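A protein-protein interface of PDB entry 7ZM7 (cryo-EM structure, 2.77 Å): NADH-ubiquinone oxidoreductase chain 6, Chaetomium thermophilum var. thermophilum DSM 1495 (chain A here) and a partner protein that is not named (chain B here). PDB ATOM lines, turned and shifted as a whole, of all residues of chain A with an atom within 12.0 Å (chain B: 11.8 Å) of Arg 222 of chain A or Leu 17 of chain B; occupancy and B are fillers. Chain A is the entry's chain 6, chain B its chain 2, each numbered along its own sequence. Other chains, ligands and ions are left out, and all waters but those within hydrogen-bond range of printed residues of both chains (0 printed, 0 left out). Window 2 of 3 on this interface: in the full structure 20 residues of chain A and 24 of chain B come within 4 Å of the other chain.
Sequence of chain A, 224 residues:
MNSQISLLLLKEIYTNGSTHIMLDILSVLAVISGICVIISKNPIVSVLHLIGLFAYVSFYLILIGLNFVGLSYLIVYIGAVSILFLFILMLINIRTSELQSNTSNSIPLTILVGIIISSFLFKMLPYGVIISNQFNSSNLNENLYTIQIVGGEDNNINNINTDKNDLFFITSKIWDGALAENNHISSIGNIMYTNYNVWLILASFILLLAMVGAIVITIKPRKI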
ATOM      1  N   VAL A 212       3.679 -33.048 -29.179  1.00  0.00           N
ATOM      2  CA  VAL A 212       3.774 -32.282 -27.945  1.00  0.00           C
ATOM      3  C   VAL A 212       5.205 -32.262 -27.434  1.00  0.00           C
ATOM      4  O   VAL A 212       5.715 -31.217 -27.024  1.00  0.00           O
ATOM      5  CB  VAL A 212       2.811 -32.868 -26.903  1.00  0.00           C
ATOM      6  CG1 VAL A 212       3.096 -32.325 -25.522  1.00  0.00           C
ATOM      7  CG2 VAL A 212       1.388 -32.598 -27.323  1.00  0.00           C
ATOM      8  N   ILE A 215       7.743 -30.172 -29.711  1.00  0.00           N
ATOM      9  CA  ILE A 215       7.468 -28.748 -29.588  1.00  0.00           C
ATOM     10  C   ILE A 215       7.926 -28.231 -28.228  1.00  0.00           C
ATOM     11  O   ILE A 215       8.518 -27.153 -28.135  1.00  0.00           O
ATOM     12  CB  ILE A 215       5.973 -28.476 -29.850  1.00  0.00           C
ATOM     13  CG1 ILE A 215       5.687 -28.559 -31.352  1.00  0.00           C
ATOM     14  CG2 ILE A 215       5.560 -27.115 -29.321  1.00  0.00           C
ATOM     15  CD1 ILE A 215       4.216 -28.597 -31.715  1.00  0.00           C
ATOM     16  N   VAL A 216       7.702 -28.997 -27.158  1.00  0.00           N
ATOM     17  CA  VAL A 216       7.995 -28.496 -25.820  1.00  0.00           C
ATOM     18  C   VAL A 216       9.490 -28.463 -25.523  1.00  0.00           C
ATOM     19  O   VAL A 216       9.920 -27.726 -24.636  1.00  0.00           O
ATOM     20  CB  VAL A 216       7.256 -29.313 -24.737  1.00  0.00           C
ATOM     21  CG1 VAL A 216       7.809 -30.702 -24.630  1.00  0.00           C
ATOM     22  CG2 VAL A 216       7.316 -28.623 -23.398  1.00  0.00           C
ATOM     23  N   ILE A 217      10.316 -29.231 -26.232  1.00  0.00           N
ATOM     24  CA  ILE A 217      11.742 -29.220 -25.937  1.00  0.00           C
ATOM     25  C   ILE A 217      12.525 -28.312 -26.859  1.00  0.00           C
ATOM     26  O   ILE A 217      13.740 -28.198 -26.705  1.00  0.00           O
ATOM     27  CB  ILE A 217      12.350 -30.636 -25.954  1.00  0.00           C
ATOM     28  CG1 ILE A 217      12.298 -31.231 -27.355  1.00  0.00           C
ATOM     29  CG2 ILE A 217      11.682 -31.513 -24.913  1.00  0.00           C
ATOM     30  CD1 ILE A 217      13.240 -32.370 -27.580  1.00  0.00           C
ATOM     31  N   THR A 218      11.874 -27.639 -27.793  1.00  0.00           N
ATOM     32  CA  THR A 218      12.601 -26.770 -28.706  1.00  0.00           C
ATOM     33  C   THR A 218      12.202 -25.308 -28.594  1.00  0.00           C
ATOM     34  O   THR A 218      13.080 -24.444 -28.586  1.00  0.00           O
ATOM     35  CB  THR A 218      12.455 -27.254 -30.167  1.00  0.00           C
ATOM     36  OG1 THR A 218      11.089 -27.564 -30.453  1.00  0.00           O
ATOM     37  CG2 THR A 218      13.327 -28.464 -30.425  1.00  0.00           C
ATOM     38  N   ILE A 219      10.933 -24.988 -28.513  1.00  0.00           N
ATOM     39  CA  ILE A 219      10.549 -23.601 -28.672  1.00  0.00           C
ATOM     40  C   ILE A 219      10.624 -22.906 -27.323  1.00  0.00           C
ATOM     41  O   ILE A 219      10.474 -23.513 -26.267  1.00  0.00           O
ATOM     42  CB  ILE A 219       9.150 -23.416 -29.287  1.00  0.00           C
ATOM     43  CG1 ILE A 219       8.063 -23.990 -28.397  1.00  0.00           C
ATOM     44  CG2 ILE A 219       9.067 -24.110 -30.628  1.00  0.00           C
ATOM     45  CD1 ILE A 219       6.688 -23.605 -28.870  1.00  0.00           C
ATOM     46  N   LYS A 220      10.891 -21.614 -27.372  1.00  0.00           N
ATOM     47  CA  LYS A 220      10.717 -20.748 -26.228  1.00  0.00           C
ATOM     48  C   LYS A 220       9.249 -20.363 -26.150  1.00  0.00           C
ATOM     49  O   LYS A 220       8.718 -19.821 -27.122  1.00  0.00           O
ATOM     50  CB  LYS A 220      11.586 -19.513 -26.372  1.00  0.00           C
ATOM     51  CG  LYS A 220      11.436 -18.471 -25.297  1.00  0.00           C
ATOM     52  CD  LYS A 220      12.056 -18.906 -23.998  1.00  0.00           C
ATOM     53  CE  LYS A 220      11.800 -17.878 -22.915  1.00  0.00           C
ATOM     54  NZ  LYS A 220      12.482 -16.588 -23.216  1.00  0.00           N
ATOM     55  N   PRO A 221       8.551 -20.649 -25.056  1.00  0.00           N
ATOM     56  CA  PRO A 221       7.125 -20.311 -24.992  1.00  0.00           C
ATOM     57  C   PRO A 221       6.901 -18.813 -25.111  1.00  0.00           C
ATOM     58  O   PRO A 221       7.686 -18.004 -24.612  1.00  0.00           O
ATOM     59  CB  PRO A 221       6.694 -20.833 -23.615  1.00  0.00           C
ATOM     60  CG  PRO A 221       7.745 -21.788 -23.218  1.00  0.00           C
ATOM     61  CD  PRO A 221       9.014 -21.299 -23.823  1.00  0.00           C
ATOM     62  N   ARG A 222       5.812 -18.453 -25.782  1.00  0.00           N
ATOM     63  CA  ARG A 222       5.449 -17.056 -26.008  1.00  0.00           C
ATOM     64  C   ARG A 222       6.556 -16.303 -26.735  1.00  0.00           C
ATOM     65  O   ARG A 222       6.384 -15.144 -27.111  1.00  0.00           O
ATOM     66  CB  ARG A 222       5.121 -16.357 -24.685  1.00  0.00           C
ATOM     67  N   LEU B   9      -6.558 -33.112 -20.425  1.00  0.00           N
ATOM     68  CA  LEU B   9      -5.415 -32.311 -19.935  1.00  0.00           C
ATOM     69  C   LEU B   9      -4.726 -31.659 -21.133  1.00  0.00           C
ATOM     70  O   LEU B   9      -4.310 -30.496 -21.007  1.00  0.00           O
ATOM     71  CB  LEU B   9      -4.473 -33.221 -19.148  1.00  0.00           C
ATOM     72  CG  LEU B   9      -3.265 -32.546 -18.500  1.00  0.00           C
ATOM     73  CD1 LEU B   9      -3.705 -31.436 -17.562  1.00  0.00           C
ATOM     74  CD2 LEU B   9      -2.416 -33.558 -17.750  1.00  0.00           C
ATOM     75  N   LEU B  10      -4.611 -32.383 -22.248  1.00  0.00           N
ATOM     76  CA  LEU B  10      -3.926 -31.839 -23.442  1.00  0.00           C
ATOM     77  C   LEU B  10      -4.694 -30.619 -23.945  1.00  0.00           C
ATOM     78  O   LEU B  10      -4.052 -29.595 -24.159  1.00  0.00           O
ATOM     79  CB  LEU B  10      -3.827 -32.923 -24.515  1.00  0.00           C
ATOM     80  CG  LEU B  10      -3.160 -32.513 -25.825  1.00  0.00           C
ATOM     81  CD1 LEU B  10      -1.817 -31.849 -25.578  1.00  0.00           C
ATOM     82  CD2 LEU B  10      -2.990 -33.723 -26.721  1.00  0.00           C
ATOM     83  N   LEU B  11      -6.019 -30.707 -24.009  1.00  0.00           N
ATOM     84  CA  LEU B  11      -6.833 -29.589 -24.519  1.00  0.00           C
ATOM     85  C   LEU B  11      -6.656 -28.376 -23.617  1.00  0.00           C
ATOM     86  O   LEU B  11      -6.564 -27.270 -24.152  1.00  0.00           O
ATOM     87  CB  LEU B  11      -8.295 -30.039 -24.561  1.00  0.00           C
ATOM     88  CG  LEU B  11      -9.072 -29.677 -25.823  1.00  0.00           C
ATOM     89  CD1 LEU B  11      -8.194 -29.797 -27.053  1.00  0.00           C
ATOM     90  CD2 LEU B  11     -10.300 -30.559 -25.960  1.00  0.00           C
ATOM     91  N   SER B  12      -6.649 -28.577 -22.301  1.00  0.00           N
ATOM     92  CA  SER B  12      -6.501 -27.459 -21.336  1.00  0.00           C
ATOM     93  C   SER B  12      -5.119 -26.812 -21.419  1.00  0.00           C
ATOM     94  O   SER B  12      -5.060 -25.580 -21.423  1.00  0.00           O
ATOM     95  CB  SER B  12      -6.858 -27.883 -19.944  1.00  0.00           C
ATOM     96  OG  SER B  12      -8.253 -27.760 -19.726  1.00  0.00           O
ATOM     97  N   THR B  13      -4.055 -27.611 -21.506  1.00  0.00           N
ATOM     98  CA  THR B  13      -2.671 -27.068 -21.548  1.00  0.00           C
ATOM     99  C   THR B  13      -2.396 -26.507 -22.943  1.00  0.00           C
ATOM    100  O   THR B  13      -1.383 -25.819 -23.100  1.00  0.00           O
ATOM    101  CB  THR B  13      -1.658 -28.159 -21.185  1.00  0.00           C
ATOM    102  OG1 THR B  13      -2.239 -28.962 -20.158  1.00  0.00           O
ATOM    103  CG2 THR B  13      -0.326 -27.617 -20.715  1.00  0.00           C
ATOM    104  N   SER B  14      -3.279 -26.763 -23.903  1.00  0.00           N
ATOM    105  CA  SER B  14      -3.062 -26.357 -25.307  1.00  0.00           C
ATOM    106  C   SER B  14      -3.512 -24.912 -25.450  1.00  0.00           C
ATOM    107  O   SER B  14      -2.920 -24.191 -26.254  1.00  0.00           O
ATOM    108  CB  SER B  14      -3.853 -27.230 -26.214  1.00  0.00           C
ATOM    109  OG  SER B  14      -3.315 -28.533 -26.299  1.00  0.00           O
ATOM    110  N   VAL B  15      -4.513 -24.519 -24.669  1.00  0.00           N
ATOM    111  CA  VAL B  15      -5.019 -23.162 -24.796  1.00  0.00           C
ATOM    112  C   VAL B  15      -4.456 -22.224 -23.744  1.00  0.00           C
ATOM    113  O   VAL B  15      -4.874 -21.063 -23.680  1.00  0.00           O
ATOM    114  CB  VAL B  15      -6.558 -23.132 -24.728  1.00  0.00           C
ATOM    115  CG1 VAL B  15      -7.150 -23.967 -25.833  1.00  0.00           C
ATOM    116  CG2 VAL B  15      -7.051 -23.585 -23.380  1.00  0.00           C
ATOM    117  N   THR B  16      -3.524 -22.679 -22.921  1.00  0.00           N
ATOM    118  CA  THR B  16      -2.891 -21.825 -21.931  1.00  0.00           C
ATOM    119  C   THR B  16      -1.400 -21.746 -22.197  1.00  0.00           C
ATOM    120  O   THR B  16      -0.808 -22.657 -22.775  1.00  0.00           O
ATOM    121  CB  THR B  16      -3.127 -22.325 -20.497  1.00  0.00           C
ATOM    122  OG1 THR B  16      -2.792 -21.285 -19.574  1.00  0.00           O
ATOM    123  CG2 THR B  16      -2.270 -23.531 -20.193  1.00  0.00           C
ATOM    124  N   LEU B  17      -0.802 -20.629 -21.776  1.00  0.00           N
ATOM    125  CA  LEU B  17       0.670 -20.469 -21.876  1.00  0.00           C
ATOM    126  C   LEU B  17       1.174 -20.083 -20.484  1.00  0.00           C
ATOM    127  O   LEU B  17       2.376 -19.815 -20.352  1.00  0.00           O
ATOM    128  CB  LEU B  17       0.973 -19.364 -22.890  1.00  0.00           C
ATOM    129  CG  LEU B  17       1.636 -19.814 -24.191  1.00  0.00           C
ATOM    130  CD1 LEU B  17       0.677 -20.629 -25.041  1.00  0.00           C
ATOM    131  CD2 LEU B  17       2.133 -18.617 -24.979  1.00  0.00           C
ATOM    132  N   ARG B  18       0.286 -20.058 -19.486  1.00  0.00           N
ATOM    133  CA  ARG B  18       0.667 -19.593 -18.126  1.00  0.00           C
ATOM    134  C   ARG B  18       1.454 -20.679 -17.388  1.00  0.00           C
ATOM    135  O   ARG B  18       0.944 -21.803 -17.279  1.00  0.00           O
ATOM    136  CB  ARG B  18      -0.591 -19.192 -17.350  1.00  0.00           C
ATOM    137  CG  ARG B  18      -1.206 -17.872 -17.793  1.00  0.00           C
ATOM    138  CD  ARG B  18      -2.584 -17.667 -17.191  1.00  0.00           C
ATOM    139  NE  ARG B  18      -2.570 -17.688 -15.737  1.00  0.00           N
ATOM    140  CZ  ARG B  18      -3.648 -17.572 -14.970  1.00  0.00           C
ATOM    141  NH1 ARG B  18      -4.840 -17.429 -15.521  1.00  0.00           N
ATOM    142  NH2 ARG B  18      -3.531 -17.599 -13.655  1.00  0.00           N
ATOM    143  N   ARG B  19       2.637 -20.331 -16.871  1.00  0.00           N
ATOM    144  CA  ARG B  19       3.497 -21.327 -16.185  1.00  0.00           C
ATOM    145  C   ARG B  19       3.074 -21.452 -14.723  1.00  0.00           C
ATOM    146  O   ARG B  19       3.380 -22.504 -14.149  1.00  0.00           O
ATOM    147  CB  ARG B  19       4.979 -20.965 -16.326  1.00  0.00           C
ATOM    148  CG  ARG B  19       5.515 -21.079 -17.744  1.00  0.00           C
ATOM    149  CD  ARG B  19       7.002 -20.794 -17.782  1.00  0.00           C
ATOM    150  NE  ARG B  19       7.321 -19.615 -16.994  1.00  0.00           N
ATOM    151  CZ  ARG B  19       7.501 -18.395 -17.484  1.00  0.00           C
ATOM    152  NH1 ARG B  19       7.403 -18.180 -18.784  1.00  0.00           N
ATOM    153  NH2 ARG B  19       7.780 -17.394 -16.670  1.00  0.00           N
ATOM    154  N   ASP B  20       2.446 -20.450 -14.113  1.00  0.00           N
ATOM    155  CA  ASP B  20       1.917 -20.558 -12.762  1.00  0.00           C
ATOM    156  C   ASP B  20       0.827 -21.604 -12.666  1.00  0.00           C
ATOM    157  O   ASP B  20       0.497 -22.049 -11.569  1.00  0.00           O
ATOM    158  CB  ASP B  20       1.403 -19.187 -12.305  1.00  0.00           C
ATOM    159  CG  ASP B  20       0.186 -18.726 -13.070  1.00  0.00           C
ATOM    160  OD1 ASP B  20       0.294 -18.423 -14.264  1.00  0.00           O
ATOM    161  OD2 ASP B  20      -0.884 -18.592 -12.479  1.00  0.00           O
ATOM    162  N   MET B  21       0.447 -22.195 -13.793  1.00  0.00           N
ATOM    163  CA  MET B  21      -0.781 -23.013 -13.922  1.00  0.00           C
ATOM    164  C   MET B  21      -0.326 -24.469 -14.016  1.00  0.00           C
ATOM    165  O   MET B  21      -1.133 -25.334 -14.377  1.00  0.00           O
ATOM    166  CB  MET B  21      -1.510 -22.571 -15.197  1.00  0.00           C
ATOM    167  CG  MET B  21      -2.880 -23.172 -15.426  1.00  0.00           C
ATOM    168  SD  MET B  21      -3.942 -23.121 -13.974  1.00  0.00           S
ATOM    169  CE  MET B  21      -4.994 -24.531 -14.313  1.00  0.00           C
ATOM    170  N   SER B  22       0.928 -24.742 -13.648  1.00  0.00           N
ATOM    171  CA  SER B  22       1.503 -26.109 -13.757  1.00  0.00           C
ATOM    172  C   SER B  22       1.240 -26.908 -12.483  1.00  0.00           C
ATOM    173  O   SER B  22       0.908 -28.091 -12.597  1.00  0.00           O
ATOM    174  CB  SER B  22       2.971 -26.022 -14.022  1.00  0.00           C
ATOM    175  OG  SER B  22       3.549 -25.014 -13.217  1.00  0.00           O
ATOM    176  N   ILE B  23       1.332 -26.257 -11.325  1.00  0.00           N
ATOM    177  CA  ILE B  23       1.158 -26.968 -10.030  1.00  0.00           C
ATOM    178  C   ILE B  23      -0.242 -27.582 -10.009  1.00  0.00           C
ATOM    179  O   ILE B  23      -0.362 -28.724  -9.545  1.00  0.00           O
ATOM    180  CB  ILE B  23       1.424 -26.004  -8.851  1.00  0.00           C
ATOM    181  CG1 ILE B  23       1.243 -26.678  -7.490  1.00  0.00           C
ATOM    182  CG2 ILE B  23       0.601 -24.729  -8.971  1.00  0.00           C
ATOM    183  CD1 ILE B  23       2.445 -26.552  -6.590  1.00  0.00           C
ATOM    184  N   PHE B  25      -2.173 -28.433 -12.705  1.00  0.00           N
ATOM    185  CA  PHE B  25      -2.312 -29.502 -13.731  1.00  0.00           C
ATOM    186  C   PHE B  25      -1.670 -30.793 -13.225  1.00  0.00           C
ATOM    187  O   PHE B  25      -2.092 -31.860 -13.679  1.00  0.00           O
ATOM    188  CB  PHE B  25      -1.636 -29.088 -15.038  1.00  0.00           C
ATOM    189  CG  PHE B  25      -2.447 -28.191 -15.938  1.00  0.00           C
ATOM    190  CD1 PHE B  25      -3.831 -28.183 -15.878  1.00  0.00           C
ATOM    191  CD2 PHE B  25      -1.824 -27.371 -16.863  1.00  0.00           C
ATOM    192  CE1 PHE B  25      -4.571 -27.364 -16.714  1.00  0.00           C
ATOM    193  CE2 PHE B  25      -2.566 -26.550 -17.695  1.00  0.00           C
ATOM    194  CZ  PHE B  25      -3.938 -26.549 -17.621  1.00  0.00           C
ATOM    195  N   MET B 116       8.571 -19.945  -8.120  1.00  0.00           N
ATOM    196  CA  MET B 116       9.028 -19.955  -9.501  1.00  0.00           C
ATOM    197  C   MET B 116      10.245 -20.850  -9.718  1.00  0.00           C
ATOM    198  O   MET B 116      11.079 -20.557 -10.577  1.00  0.00           O
ATOM    199  CB  MET B 116       9.322 -18.538 -10.003  1.00  0.00           C
ATOM    200  CG  MET B 116       8.107 -17.703 -10.376  1.00  0.00           C
ATOM    201  SD  MET B 116       7.001 -16.992  -9.148  1.00  0.00           S
ATOM    202  CE  MET B 116       7.976 -15.637  -8.529  1.00  0.00           C
ATOM    203  N   MET B 120       8.510 -26.348 -10.977  1.00  0.00           N
ATOM    204  CA  MET B 120       7.158 -25.791 -10.803  1.00  0.00           C
ATOM    205  C   MET B 120       6.727 -25.020 -12.050  1.00  0.00           C
ATOM    206  O   MET B 120       5.679 -24.390 -11.974  1.00  0.00           O
ATOM    207  CB  MET B 120       7.128 -24.864  -9.583  1.00  0.00           C
ATOM    208  CG  MET B 120       7.155 -25.611  -8.275  1.00  0.00           C
ATOM    209  SD  MET B 120       5.890 -26.900  -8.266  1.00  0.00           S
ATOM    210  CE  MET B 120       6.352 -27.800  -6.793  1.00  0.00           C
ATOM    211  N   LYS B 121       7.484 -25.058 -13.149  1.00  0.00           N
ATOM    212  CA  LYS B 121       7.145 -24.171 -14.300  1.00  0.00           C
ATOM    213  C   LYS B 121       6.817 -24.938 -15.585  1.00  0.00           C
ATOM    214  O   LYS B 121       5.963 -24.440 -16.335  1.00  0.00           O
ATOM    215  CB  LYS B 121       8.226 -23.106 -14.505  1.00  0.00           C
ATOM    216  CG  LYS B 121       8.255 -22.032 -13.427  1.00  0.00           C
ATOM    217  CD  LYS B 121       9.369 -21.035 -13.591  1.00  0.00           C
ATOM    218  CE  LYS B 121       8.896 -19.691 -14.097  1.00  0.00           C
ATOM    219  NZ  LYS B 121      10.031 -18.794 -14.412  1.00  0.00           N
ATOM    220  N   ILE B 122       7.451 -26.080 -15.852  1.00  0.00           N
ATOM    221  CA  ILE B 122       7.045 -26.849 -17.066  1.00  0.00           C
ATOM    222  C   ILE B 122       5.557 -27.191 -16.928  1.00  0.00           C
ATOM    223  O   ILE B 122       5.154 -27.587 -15.837  1.00  0.00           O
ATOM    224  CB  ILE B 122       7.923 -28.102 -17.236  1.00  0.00           C
ATOM    225  CG1 ILE B 122       9.386 -27.812 -16.891  1.00  0.00           C
ATOM    226  CG2 ILE B 122       7.772 -28.674 -18.635  1.00  0.00           C
ATOM    227  CD1 ILE B 122      10.280 -29.027 -16.912  1.00  0.00           C
ATOM    228  N   ILE B 123       4.789 -26.975 -18.087  1.00  0.00           N
ATOM    229  CA  ILE B 123       3.310 -27.169 -17.992  1.00  0.00           C
ATOM    230  C   ILE B 123       2.968 -28.539 -18.563  1.00  0.00           C
ATOM    231  O   ILE B 123       1.924 -29.098 -18.196  1.00  0.00           O
ATOM    232  CB  ILE B 123       2.540 -26.050 -18.721  1.00  0.00           C
ATOM    233  CG1 ILE B 123       3.205 -24.708 -18.467  1.00  0.00           C
ATOM    234  CG2 ILE B 123       1.111 -25.996 -18.221  1.00  0.00           C
ATOM    235  CD1 ILE B 123       2.964 -24.301 -17.059  1.00  0.00           C
ATOM    236  N   GLU B 124       3.844 -29.092 -19.338  1.00  0.00           N
ATOM    237  CA  GLU B 124       3.577 -30.362 -20.063  1.00  0.00           C
ATOM    238  C   GLU B 124       4.165 -31.535 -19.282  1.00  0.00           C
ATOM    239  O   GLU B 124       3.987 -32.669 -19.722  1.00  0.00           O
ATOM    240  CB  GLU B 124       4.146 -30.292 -21.482  1.00  0.00           C
ATOM    241  CG  GLU B 124       3.395 -29.327 -22.380  1.00  0.00           C
ATOM    242  CD  GLU B 124       3.679 -27.848 -22.169  1.00  0.00           C
ATOM    243  OE1 GLU B 124       4.715 -27.522 -21.553  1.00  0.00           O
ATOM    244  OE2 GLU B 124       2.858 -27.026 -22.615  1.00  0.00           O
ATOM    245  N   ARG B 167      15.228 -27.893 -20.703  1.00  0.00           N
ATOM    246  CA  ARG B 167      15.845 -27.506 -22.001  1.00  0.00           C
ATOM    247  C   ARG B 167      17.039 -26.588 -21.804  1.00  0.00           C
ATOM    248  O   ARG B 167      17.833 -26.456 -22.737  1.00  0.00           O
ATOM    249  CB  ARG B 167      14.765 -26.898 -22.901  1.00  0.00           C
ATOM    250  CG  ARG B 167      13.984 -25.745 -22.293  1.00  0.00           C
ATOM    251  CD  ARG B 167      12.919 -25.302 -23.279  1.00  0.00           C
ATOM    252  NE  ARG B 167      13.483 -25.014 -24.588  1.00  0.00           N
ATOM    253  CZ  ARG B 167      13.860 -23.812 -25.005  1.00  0.00           C
ATOM    254  NH1 ARG B 167      14.366 -23.668 -26.216  1.00  0.00           N
ATOM    255  NH2 ARG B 167      13.724 -22.760 -24.221  1.00  0.00           N
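The guanidinium group of Arg 167 of chain B lies within hydrogen-bond range of the backbone carbonyl oxygen of Thr 218 of chain A (2.8 Å).
The backbone carbonyl oxygen (O) of Leu 10 of chain B is in hydrogen-bond range of the side-chain hydroxyl (OG) of Ser 14 of chain B. The backbone carbonyl oxygen (O) of Ile 215 of chain A lies within hydrogen-bond range of the side-chain hydroxyl (OG1) of Thr 218 of chain A (3.5 Å).
Of the 9 printed residues of chain A, 6 touch a printed residue of chain B. Printed residues of chain A that touch a printed residue of chain B: Val 212, Val 216, Ile 217, Thr 218, Ile 219 and Arg 222. Hydrophobic or aromatic side chains of chain A that line the printed part of chain B: Val 212 and Val 216. Among the printed residues, 6 pairs touch across the chains. Among the printed residues, no Asp or Glu carboxylate lies within 4 Å of a Lys or Arg side-chain nitrogen of the other chain.
Arg 222 of chain A touches just one residue of chain B: Leu 17. Of chain A, only Arg 222 (3.8 Å) comes within 4 Å of Leu 17 of chain B. No residue of chain B comes within 4 Å of Lys 220 of chain A. No residue of chain B comes within 4 Å of Pro 221 of chain A. No residue of chain A comes within 4 Å of Thr 16 of chain B. No residue of chain A comes within 4 Å of Arg 19 of chain B. Of the printed residues of chain A, Leu 10 of chain B touches Val 212. Of the printed residues of chain A, Glu 124 of chain B touches Val 216. Met 120 of chain B touches none of the printed residues of chain A. Arg 18 of chain B touches none of the printed residues of chain A. The nearest printed residue of chain B that does not touch Ile 217 of chain A is Glu 124 of chain B (7.5 Å).
Among the printed residues, merely in contact across the chains: Val 212 of chain A with Leu 10 of chain B (3.7 Å), Val 216 of chain A with Glu 124 of chain B (3.4 Å), Ile 217 of chain A with Arg 167 of chain B (3.8 Å), Ile 219 of chain A with Arg 167 of chain B (3.6 Å) and Arg 222 of chain A with Leu 17 of chain B (3.8 Å).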
